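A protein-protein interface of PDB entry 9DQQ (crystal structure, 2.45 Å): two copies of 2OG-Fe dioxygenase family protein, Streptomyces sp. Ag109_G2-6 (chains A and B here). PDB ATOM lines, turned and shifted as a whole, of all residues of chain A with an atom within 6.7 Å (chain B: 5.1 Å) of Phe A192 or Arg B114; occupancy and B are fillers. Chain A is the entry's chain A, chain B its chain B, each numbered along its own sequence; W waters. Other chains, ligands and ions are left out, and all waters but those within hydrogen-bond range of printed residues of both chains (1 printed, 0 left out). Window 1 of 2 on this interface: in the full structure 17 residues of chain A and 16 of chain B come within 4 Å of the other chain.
Water W1 lies within hydrogen-bond range of the guanidinium group (NH1) of Arg B114 and the side-chain carboxylate (OE2) of Glu A178.
The side-chain hydroxyl (OH) of Tyr A14 sits at hydrogen-bond distance from the side-chain carboxylate (OE2) of Glu B70 (2.4 Å).
The side-chain carboxylate (OE2) of Glu A178 lies within salt-bridge range of the guanidinium group (NE) of Arg B111 (2.8 Å).
O of Glu A191 lies within hydrogen-bond range of N of Val B71, at 2.6 Å.
OE1 of Glu A191 sits at hydrogen-bond distance from OG1 of Thr B110, 2.9 Å away.
The guanidinium group (NH1) of Arg B114 lies within salt-bridge range of the side-chain carboxylate (OE1) of Glu A191, at 2.6 Å.
The backbone NH (N) of Cys A193 lies within hydrogen-bond range of the backbone carbonyl oxygen (O) of Thr B68.
The guanidinium group of Arg B114 sits at hydrogen-bond distance from the side-chain sulfur of Cys A193.
The backbone carbonyl oxygen (O) of Glu A191 sits close to the backbone carbonyl oxygen (O) of Gly B69, at 3.2 Å.
No position is printed for both chains.
Of the 16 printed residues of chain A, 7 touch a printed residue of chain B.
Printed residues of chain A that touch a printed residue of chain B: Tyr A14, Leu A16, Glu A178, Ala A190, Glu A191, Phe A192 and Cys A193.
Hydrophobic or aromatic side chains of chain A that line the printed part of chain B: Tyr A14, Leu A16, Ala A190 and Phe A192.
Of the 15 printed residues of chain B, 7 touch a printed residue of chain A.
Among the printed residues, pairs that only touch across the chains: Glu A191 with Glu B70, Ala A190 with Val B71, Phe A192 with Gly B69, Phe A192 with Thr B68, Leu A16 with Thr B68, Phe A192 with Arg B114, Phe A192 with Glu B70, Leu A16 with Glu B70 and Glu A178 with Arg B114.
Phe A192 touches just these residues of chain B: Thr B68, Gly B69, Glu B70 and Arg B114.
Printed residues of chain A within 4 Å of Arg B114: Glu A178 (3.8 Å), Glu A191 (2.6 Å), Phe A192 (3.7 Å) and Cys A193 (3.3 Å).
Of the printed residues of chain B, Tyr A14 touches Glu B70.
Of the printed residues of chain B, Glu A191 touches Gly B69, Glu B70, Val B71, Thr B110 and Arg B114.
Leu B112 touches none of the printed residues of chain A.
The nearest printed residue of chain A that does not touch Thr B68 is Leu A194 (5.0 Å).
The backbone NH of Ser A179 sits at hydrogen-bond distance from the backbone carbonyl oxygen of Phe A192 (3.0 Å).
The side-chain carboxylate (OE2) of Glu A191 is in hydrogen-bond range of the side-chain amide nitrogen (NE2) of Gln A180, 2.8 Å away.
The backbone carbonyl oxygen (O) of Ala A190 is in hydrogen-bond range of the backbone NH (N) of Val A181.
OG1 of Thr B68 lies close to N of Glu B70.
The backbone carbonyl oxygen of Gly B69 lies within hydrogen-bond range of the guanidinium group of Arg B114 (2.8 Å).
The side-chain hydroxyl of Thr B110 sits at hydrogen-bond distance from the guanidinium group of Arg B114, at 3.1 Å.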
ATOM      1  N   TYR A  14      11.783   5.095  38.607  1.00  0.00           N
ATOM      2  CA  TYR A  14      10.495   5.743  38.817  1.00  0.00           C
ATOM      3  C   TYR A  14       9.424   4.688  38.606  1.00  0.00           C
ATOM      4  O   TYR A  14       9.681   3.639  38.021  1.00  0.00           O
ATOM      5  CB  TYR A  14      10.264   6.940  37.868  1.00  0.00           C
ATOM      6  CG  TYR A  14      10.045   6.517  36.424  1.00  0.00           C
ATOM      7  CD1 TYR A  14      11.124   6.249  35.586  1.00  0.00           C
ATOM      8  CD2 TYR A  14       8.762   6.369  35.909  1.00  0.00           C
ATOM      9  CE1 TYR A  14      10.928   5.859  34.267  1.00  0.00           C
ATOM     10  CE2 TYR A  14       8.553   5.982  34.591  1.00  0.00           C
ATOM     11  CZ  TYR A  14       9.640   5.724  33.771  1.00  0.00           C
ATOM     12  OH  TYR A  14       9.429   5.325  32.456  1.00  0.00           O
ATOM     13  N   SER A  15       8.219   4.978  39.091  1.00  0.00           N
ATOM     14  CA  SER A  15       7.079   4.080  38.937  1.00  0.00           C
ATOM     15  C   SER A  15       5.803   4.902  38.973  1.00  0.00           C
ATOM     16  O   SER A  15       5.715   5.883  39.713  1.00  0.00           O
ATOM     17  CB  SER A  15       7.038   3.015  40.034  1.00  0.00           C
ATOM     18  OG  SER A  15       5.735   2.502  40.194  1.00  0.00           O
ATOM     19  N   LEU A  16       4.813   4.487  38.194  1.00  0.00           N
ATOM     20  CA  LEU A  16       3.584   5.246  38.028  1.00  0.00           C
ATOM     21  C   LEU A  16       2.420   4.501  38.658  1.00  0.00           C
ATOM     22  O   LEU A  16       2.350   3.276  38.607  1.00  0.00           O
ATOM     23  CB  LEU A  16       3.290   5.500  36.544  1.00  0.00           C
ATOM     24  CG  LEU A  16       4.455   6.149  35.789  1.00  0.00           C
ATOM     25  CD1 LEU A  16       4.141   6.303  34.302  1.00  0.00           C
ATOM     26  CD2 LEU A  16       4.824   7.488  36.400  1.00  0.00           C
ATOM     27  N   ILE A 166       5.083  12.067  44.344  1.00  0.00           N
ATOM     28  CA  ILE A 166       4.301  13.218  43.952  1.00  0.00           C
ATOM     29  C   ILE A 166       2.905  12.716  43.660  1.00  0.00           C
ATOM     30  O   ILE A 166       2.731  11.734  42.937  1.00  0.00           O
ATOM     31  CB  ILE A 166       4.904  13.981  42.745  1.00  0.00           C
ATOM     32  CG1 ILE A 166       3.932  15.045  42.245  1.00  0.00           C
ATOM     33  CG2 ILE A 166       5.278  13.048  41.613  1.00  0.00           C
ATOM     34  CD1 ILE A 166       4.549  15.991  41.262  1.00  0.00           C
ATOM     35  N   GLY A 177       2.561  20.615  31.400  1.00  0.00           N
ATOM     36  CA  GLY A 177       2.857  20.045  32.706  1.00  0.00           C
ATOM     37  C   GLY A 177       3.240  18.588  32.677  1.00  0.00           C
ATOM     38  O   GLY A 177       2.887  17.839  33.595  1.00  0.00           O
ATOM     39  N   GLU A 178       3.966  18.174  31.655  1.00  0.00           N
ATOM     40  CA  GLU A 178       4.468  16.810  31.557  1.00  0.00           C
ATOM     41  C   GLU A 178       5.672  16.636  32.477  1.00  0.00           C
ATOM     42  O   GLU A 178       6.552  17.491  32.527  1.00  0.00           O
ATOM     43  CB  GLU A 178       4.872  16.501  30.112  1.00  0.00           C
ATOM     44  CG  GLU A 178       3.737  16.472  29.107  1.00  0.00           C
ATOM     45  CD  GLU A 178       3.337  17.848  28.585  1.00  0.00           C
ATOM     46  OE1 GLU A 178       3.851  18.884  29.060  1.00  0.00           O
ATOM     47  OE2 GLU A 178       2.493  17.880  27.672  1.00  0.00           O
ATOM     48  N   SER A 179       5.723  15.532  33.205  1.00  0.00           N
ATOM     49  CA  SER A 179       6.849  15.269  34.103  1.00  0.00           C
ATOM     50  C   SER A 179       7.921  14.539  33.301  1.00  0.00           C
ATOM     51  O   SER A 179       7.625  13.551  32.614  1.00  0.00           O
ATOM     52  CB  SER A 179       6.419  14.417  35.310  1.00  0.00           C
ATOM     53  OG  SER A 179       5.167  14.788  35.811  1.00  0.00           O
ATOM     54  N   GLN A 180       9.163  14.990  33.403  1.00  0.00           N
ATOM     55  CA  GLN A 180      10.243  14.400  32.619  1.00  0.00           C
ATOM     56  C   GLN A 180      11.188  13.635  33.533  1.00  0.00           C
ATOM     57  O   GLN A 180      11.599  14.154  34.574  1.00  0.00           O
ATOM     58  CB  GLN A 180      11.007  15.468  31.837  1.00  0.00           C
ATOM     59  CG  GLN A 180      10.130  16.451  31.138  1.00  0.00           C
ATOM     60  CD  GLN A 180      10.733  16.910  29.826  1.00  0.00           C
ATOM     61  OE1 GLN A 180      11.860  17.391  29.798  1.00  0.00           O
ATOM     62  NE2 GLN A 180       9.999  16.733  28.726  1.00  0.00           N
ATOM     63  N   VAL A 181      11.523  12.403  33.148  1.00  0.00           N
ATOM     64  CA  VAL A 181      12.558  11.613  33.810  1.00  0.00           C
ATOM     65  C   VAL A 181      13.820  11.647  32.955  1.00  0.00           C
ATOM     66  O   VAL A 181      13.795  11.270  31.774  1.00  0.00           O
ATOM     67  CB  VAL A 181      12.098  10.166  34.050  1.00  0.00           C
ATOM     68  CG1 VAL A 181      13.196   9.365  34.793  1.00  0.00           C
ATOM     69  CG2 VAL A 181      10.774  10.139  34.812  1.00  0.00           C
ATOM     70  N   ALA A 190      12.196   9.323  29.953  1.00  0.00           N
ATOM     71  CA  ALA A 190      10.758   9.097  30.027  1.00  0.00           C
ATOM     72  C   ALA A 190      10.014  10.403  30.234  1.00  0.00           C
ATOM     73  O   ALA A 190      10.592  11.443  30.571  1.00  0.00           O
ATOM     74  CB  ALA A 190      10.378   8.106  31.129  1.00  0.00           C
ATOM     75  N   GLU A 191       8.709  10.325  30.000  1.00  0.00           N
ATOM     76  CA  GLU A 191       7.820  11.465  30.119  1.00  0.00           C
ATOM     77  C   GLU A 191       6.407  10.921  30.209  1.00  0.00           C
ATOM     78  O   GLU A 191       6.048  10.004  29.467  1.00  0.00           O
ATOM     79  CB  GLU A 191       7.970  12.426  28.935  1.00  0.00           C
ATOM     80  CG  GLU A 191       7.263  13.744  29.162  1.00  0.00           C
ATOM     81  CD  GLU A 191       7.037  14.504  27.870  1.00  0.00           C
ATOM     82  OE1 GLU A 191       5.987  14.268  27.219  1.00  0.00           O
ATOM     83  OE2 GLU A 191       7.918  15.320  27.514  1.00  0.00           O
ATOM     84  N   PHE A 192       5.624  11.479  31.130  1.00  0.00           N
ATOM     85  CA  PHE A 192       4.296  10.984  31.479  1.00  0.00           C
ATOM     86  C   PHE A 192       3.455  12.167  31.982  1.00  0.00           C
ATOM     87  O   PHE A 192       3.946  13.292  32.170  1.00  0.00           O
ATOM     88  CB  PHE A 192       4.380   9.854  32.520  1.00  0.00           C
ATOM     89  CG  PHE A 192       5.128  10.232  33.761  1.00  0.00           C
ATOM     90  CD1 PHE A 192       6.513  10.162  33.802  1.00  0.00           C
ATOM     91  CD2 PHE A 192       4.444  10.683  34.889  1.00  0.00           C
ATOM     92  CE1 PHE A 192       7.203  10.535  34.950  1.00  0.00           C
ATOM     93  CE2 PHE A 192       5.105  11.039  36.006  1.00  0.00           C
ATOM     94  CZ  PHE A 192       6.498  10.979  36.048  1.00  0.00           C
ATOM     95  N   CYS A 193       2.176  11.918  32.203  1.00  0.00           N
ATOM     96  CA  CYS A 193       1.236  12.987  32.521  1.00  0.00           C
ATOM     97  C   CYS A 193       0.429  12.615  33.748  1.00  0.00           C
ATOM     98  O   CYS A 193      -0.407  11.705  33.698  1.00  0.00           O
ATOM     99  CB  CYS A 193       0.297  13.248  31.351  1.00  0.00           C
ATOM    100  SG  CYS A 193       1.153  13.528  29.826  1.00  0.00           S
ATOM    101  N   LEU A 194       0.654  13.337  34.836  1.00  0.00           N
ATOM    102  CA  LEU A 194      -0.325  13.322  35.912  1.00  0.00           C
ATOM    103  C   LEU A 194      -1.516  14.167  35.472  1.00  0.00           C
ATOM    104  O   LEU A 194      -1.388  15.384  35.308  1.00  0.00           O
ATOM    105  CB  LEU A 194       0.302  13.827  37.207  1.00  0.00           C
ATOM    106  CG  LEU A 194       1.632  13.123  37.528  1.00  0.00           C
ATOM    107  CD1 LEU A 194       2.202  13.653  38.803  1.00  0.00           C
ATOM    108  CD2 LEU A 194       1.451  11.635  37.615  1.00  0.00           C
ATOM    109  N   THR A 200      -0.146   9.335  40.625  1.00  0.00           N
ATOM    110  CA  THR A 200       0.964   9.280  41.556  1.00  0.00           C
ATOM    111  C   THR A 200       2.219   8.802  40.858  1.00  0.00           C
ATOM    112  O   THR A 200       2.167   7.981  39.946  1.00  0.00           O
ATOM    113  CB  THR A 200       0.608   8.378  42.727  1.00  0.00           C
ATOM    114  OG1 THR A 200      -0.427   9.005  43.481  1.00  0.00           O
ATOM    115  CG2 THR A 200       1.816   8.120  43.630  1.00  0.00           C
ATOM    116  N   MET A 201       3.351   9.329  41.298  1.00  0.00           N
ATOM    117  CA  MET A 201       4.635   8.933  40.750  1.00  0.00           C
ATOM    118  C   MET A 201       5.649   8.827  41.871  1.00  0.00           C
ATOM    119  O   MET A 201       5.839   9.796  42.619  1.00  0.00           O
ATOM    120  CB  MET A 201       5.117   9.940  39.714  1.00  0.00           C
ATOM    121  CG  MET A 201       6.301   9.423  38.952  1.00  0.00           C
ATOM    122  SD  MET A 201       7.839  10.085  39.547  1.00  0.00           S
ATOM    123  CE  MET A 201       7.624  11.829  39.193  1.00  0.00           C
ATOM    124  N   PHE B  64       4.808   3.457  24.933  1.00  0.00           N
ATOM    125  CA  PHE B  64       3.690   4.346  25.237  1.00  0.00           C
ATOM    126  C   PHE B  64       2.647   3.634  26.085  1.00  0.00           C
ATOM    127  O   PHE B  64       2.264   2.502  25.776  1.00  0.00           O
ATOM    128  CB  PHE B  64       3.050   4.875  23.938  1.00  0.00           C
ATOM    129  CG  PHE B  64       1.784   5.704  24.144  1.00  0.00           C
ATOM    130  CD1 PHE B  64       1.752   6.776  25.043  1.00  0.00           C
ATOM    131  CD2 PHE B  64       0.636   5.432  23.399  1.00  0.00           C
ATOM    132  CE1 PHE B  64       0.585   7.543  25.207  1.00  0.00           C
ATOM    133  CE2 PHE B  64      -0.516   6.195  23.547  1.00  0.00           C
ATOM    134  CZ  PHE B  64      -0.546   7.252  24.450  1.00  0.00           C
ATOM    135  N   THR B  68      -1.305   6.510  31.712  1.00  0.00           N
ATOM    136  CA  THR B  68      -0.364   7.403  32.351  1.00  0.00           C
ATOM    137  C   THR B  68       0.262   8.399  31.389  1.00  0.00           C
ATOM    138  O   THR B  68       0.912   9.351  31.845  1.00  0.00           O
ATOM    139  CB  THR B  68       0.730   6.581  33.027  1.00  0.00           C
ATOM    140  OG1 THR B  68       1.413   5.815  32.034  1.00  0.00           O
ATOM    141  CG2 THR B  68       0.108   5.643  34.091  1.00  0.00           C
ATOM    142  N   GLY B  69       0.089   8.201  30.079  1.00  0.00           N
ATOM    143  CA  GLY B  69       0.791   9.030  29.129  1.00  0.00           C
ATOM    144  C   GLY B  69       2.274   8.794  29.069  1.00  0.00           C
ATOM    145  O   GLY B  69       2.999   9.623  28.497  1.00  0.00           O
ATOM    146  N   GLU B  70       2.750   7.695  29.655  1.00  0.00           N
ATOM    147  CA  GLU B  70       4.178   7.410  29.657  1.00  0.00           C
ATOM    148  C   GLU B  70       4.691   7.237  28.227  1.00  0.00           C
ATOM    149  O   GLU B  70       4.127   6.488  27.432  1.00  0.00           O
ATOM    150  CB  GLU B  70       4.467   6.147  30.479  1.00  0.00           C
ATOM    151  CG  GLU B  70       5.958   5.888  30.700  1.00  0.00           C
ATOM    152  CD  GLU B  70       6.228   4.555  31.377  1.00  0.00           C
ATOM    153  OE1 GLU B  70       5.259   3.787  31.563  1.00  0.00           O
ATOM    154  OE2 GLU B  70       7.400   4.271  31.717  1.00  0.00           O
ATOM    155  N   VAL B  71       5.778   7.922  27.907  1.00  0.00           N
ATOM    156  CA  VAL B  71       6.440   7.799  26.620  1.00  0.00           C
ATOM    157  C   VAL B  71       7.935   7.650  26.875  1.00  0.00           C
ATOM    158  O   VAL B  71       8.524   8.442  27.619  1.00  0.00           O
ATOM    159  CB  VAL B  71       6.154   9.015  25.718  1.00  0.00           C
ATOM    160  CG1 VAL B  71       6.939   8.922  24.448  1.00  0.00           C
ATOM    161  CG2 VAL B  71       4.676   9.115  25.425  1.00  0.00           C
ATOM    162  N   THR B 110       5.520  14.584  21.438  1.00  0.00           N
ATOM    163  CA  THR B 110       4.795  13.662  22.304  1.00  0.00           C
ATOM    164  C   THR B 110       3.410  14.182  22.662  1.00  0.00           C
ATOM    165  O   THR B 110       2.518  13.384  22.961  1.00  0.00           O
ATOM    166  CB  THR B 110       5.592  13.360  23.584  1.00  0.00           C
ATOM    167  OG1 THR B 110       5.673  14.540  24.397  1.00  0.00           O
ATOM    168  CG2 THR B 110       6.993  12.867  23.238  1.00  0.00           C
ATOM    169  N   ARG B 111       3.190  15.495  22.623  1.00  0.00           N
ATOM    170  CA  ARG B 111       1.827  15.992  22.801  1.00  0.00           C
ATOM    171  C   ARG B 111       0.942  15.562  21.643  1.00  0.00           C
ATOM    172  O   ARG B 111      -0.178  15.078  21.861  1.00  0.00           O
ATOM    173  CB  ARG B 111       1.832  17.507  22.960  1.00  0.00           C
ATOM    174  CG  ARG B 111       2.247  17.967  24.362  1.00  0.00           C
ATOM    175  CD  ARG B 111       2.593  19.457  24.389  1.00  0.00           C
ATOM    176  NE  ARG B 111       3.093  19.820  25.707  1.00  0.00           N
ATOM    177  CZ  ARG B 111       3.524  21.023  26.043  1.00  0.00           C
ATOM    178  NH1 ARG B 111       3.526  22.019  25.180  1.00  0.00           N
ATOM    179  NH2 ARG B 111       3.972  21.227  27.276  1.00  0.00           N
ATOM    180  N   LEU B 112       1.441  15.690  20.399  1.00  0.00           N
ATOM    181  CA  LEU B 112       0.734  15.103  19.268  1.00  0.00           C
ATOM    182  C   LEU B 112       0.520  13.618  19.481  1.00  0.00           C
ATOM    183  O   LEU B 112      -0.605  13.124  19.375  1.00  0.00           O
ATOM    184  CB  LEU B 112       1.489  15.339  17.966  1.00  0.00           C
ATOM    185  CG  LEU B 112       1.280  16.732  17.396  1.00  0.00           C
ATOM    186  CD1 LEU B 112       2.185  16.938  16.213  1.00  0.00           C
ATOM    187  CD2 LEU B 112      -0.178  16.948  17.057  1.00  0.00           C
ATOM    188  N   LEU B 113       1.585  12.895  19.829  1.00  0.00           N
ATOM    189  CA  LEU B 113       1.455  11.458  20.064  1.00  0.00           C
ATOM    190  C   LEU B 113       0.304  11.147  21.005  1.00  0.00           C
ATOM    191  O   LEU B 113      -0.510  10.260  20.731  1.00  0.00           O
ATOM    192  CB  LEU B 113       2.755  10.887  20.630  1.00  0.00           C
ATOM    193  CG  LEU B 113       2.771   9.369  20.848  1.00  0.00           C
ATOM    194  CD1 LEU B 113       4.169   8.846  20.590  1.00  0.00           C
ATOM    195  CD2 LEU B 113       2.304   8.951  22.264  1.00  0.00           C
ATOM    196  N   ARG B 114       0.229  11.853  22.139  1.00  0.00           N
ATOM    197  CA  ARG B 114      -0.796  11.516  23.125  1.00  0.00           C
ATOM    198  C   ARG B 114      -2.161  11.957  22.637  1.00  0.00           C
ATOM    199  O   ARG B 114      -3.135  11.202  22.714  1.00  0.00           O
ATOM    200  CB  ARG B 114      -0.489  12.157  24.491  1.00  0.00           C
ATOM    201  CG  ARG B 114       0.772  11.670  25.194  1.00  0.00           C
ATOM    202  CD  ARG B 114       0.998  12.398  26.516  1.00  0.00           C
ATOM    203  NE  ARG B 114       2.220  11.938  27.168  1.00  0.00           N
ATOM    204  CZ  ARG B 114       3.394  12.548  27.080  1.00  0.00           C
ATOM    205  NH1 ARG B 114       3.528  13.696  26.449  1.00  0.00           N
ATOM    206  NH2 ARG B 114       4.462  11.991  27.641  1.00  0.00           N
ATOM    207  N   ALA B 115      -2.255  13.195  22.154  1.00  0.00           N
ATOM    208  CA  ALA B 115      -3.540  13.718  21.710  1.00  0.00           C
ATOM    209  C   ALA B 115      -4.106  12.885  20.562  1.00  0.00           C
ATOM    210  O   ALA B 115      -5.286  12.506  20.575  1.00  0.00           O
ATOM    211  CB  ALA B 115      -3.384  15.183  21.308  1.00  0.00           C
ATOM    212  N   ASP B 116      -3.264  12.567  19.570  1.00  0.00           N
ATOM    213  CA  ASP B 116      -3.701  11.726  18.460  1.00  0.00           C
ATOM    214  C   ASP B 116      -4.398  10.472  18.966  1.00  0.00           C
ATOM    215  O   ASP B 116      -5.471  10.102  18.479  1.00  0.00           O
ATOM    216  CB  ASP B 116      -2.508  11.336  17.577  1.00  0.00           C
ATOM    217  CG  ASP B 116      -1.943  12.508  16.789  1.00  0.00           C
ATOM    218  OD1 ASP B 116      -2.656  13.530  16.626  1.00  0.00           O
ATOM    219  OD2 ASP B 116      -0.781  12.410  16.327  1.00  0.00           O
ATOM    220  N   PHE B 117      -3.801   9.813  19.958  1.00  0.00           N
ATOM    221  CA  PHE B 117      -4.289   8.508  20.392  1.00  0.00           C
ATOM    222  C   PHE B 117      -5.730   8.561  20.895  1.00  0.00           C
ATOM    223  O   PHE B 117      -6.488   7.601  20.699  1.00  0.00           O
ATOM    224  CB  PHE B 117      -3.380   7.939  21.483  1.00  0.00           C
ATOM    225  CG  PHE B 117      -3.824   6.595  21.993  1.00  0.00           C
ATOM    226  CD1 PHE B 117      -4.748   6.494  23.030  1.00  0.00           C
ATOM    227  CD2 PHE B 117      -3.338   5.439  21.409  1.00  0.00           C
ATOM    228  CE1 PHE B 117      -5.165   5.260  23.479  1.00  0.00           C
ATOM    229  CE2 PHE B 117      -3.755   4.202  21.841  1.00  0.00           C
ATOM    230  CZ  PHE B 117      -4.670   4.109  22.878  1.00  0.00           C
ATOM    231  N   GLU B 118      -6.134   9.658  21.538  1.00  0.00           N
ATOM    232  CA  GLU B 118      -7.506   9.741  22.036  1.00  0.00           C
ATOM    233  C   GLU B 118      -8.553   9.609  20.927  1.00  0.00           C
ATOM    234  O   GLU B 118      -9.699   9.247  21.214  1.00  0.00           O
ATOM    235  CB  GLU B 118      -7.707  11.056  22.796  1.00  0.00           C
ATOM    236  CG  GLU B 118      -6.912  11.131  24.097  1.00  0.00           C
ATOM    237  CD  GLU B 118      -7.121   9.908  24.978  1.00  0.00           C
ATOM    238  OE1 GLU B 118      -8.294   9.559  25.241  1.00  0.00           O
ATOM    239  OE2 GLU B 118      -6.117   9.286  25.403  1.00  0.00           O
ATOM    240  N   TYR B 233       0.520   3.136  15.718  1.00  0.00           N
ATOM    241  CA  TYR B 233       0.283   2.663  17.076  1.00  0.00           C
ATOM    242  C   TYR B 233      -0.092   1.184  17.034  1.00  0.00           C
ATOM    243  O   TYR B 233      -1.056   0.808  16.362  1.00  0.00           O
ATOM    244  CB  TYR B 233      -0.848   3.462  17.731  1.00  0.00           C
ATOM    245  CG  TYR B 233      -0.645   4.970  17.870  1.00  0.00           C
ATOM    246  CD1 TYR B 233      -0.561   5.804  16.756  1.00  0.00           C
ATOM    247  CD2 TYR B 233      -0.602   5.564  19.128  1.00  0.00           C
ATOM    248  CE1 TYR B 233      -0.402   7.181  16.899  1.00  0.00           C
ATOM    249  CE2 TYR B 233      -0.442   6.937  19.279  1.00  0.00           C
ATOM    250  CZ  TYR B 233      -0.345   7.743  18.168  1.00  0.00           C
ATOM    251  OH  TYR B 233      -0.191   9.110  18.330  1.00  0.00           O
HETATM  252  O   HOH W   1       1.228  15.270  26.135  1.00  0.00           O
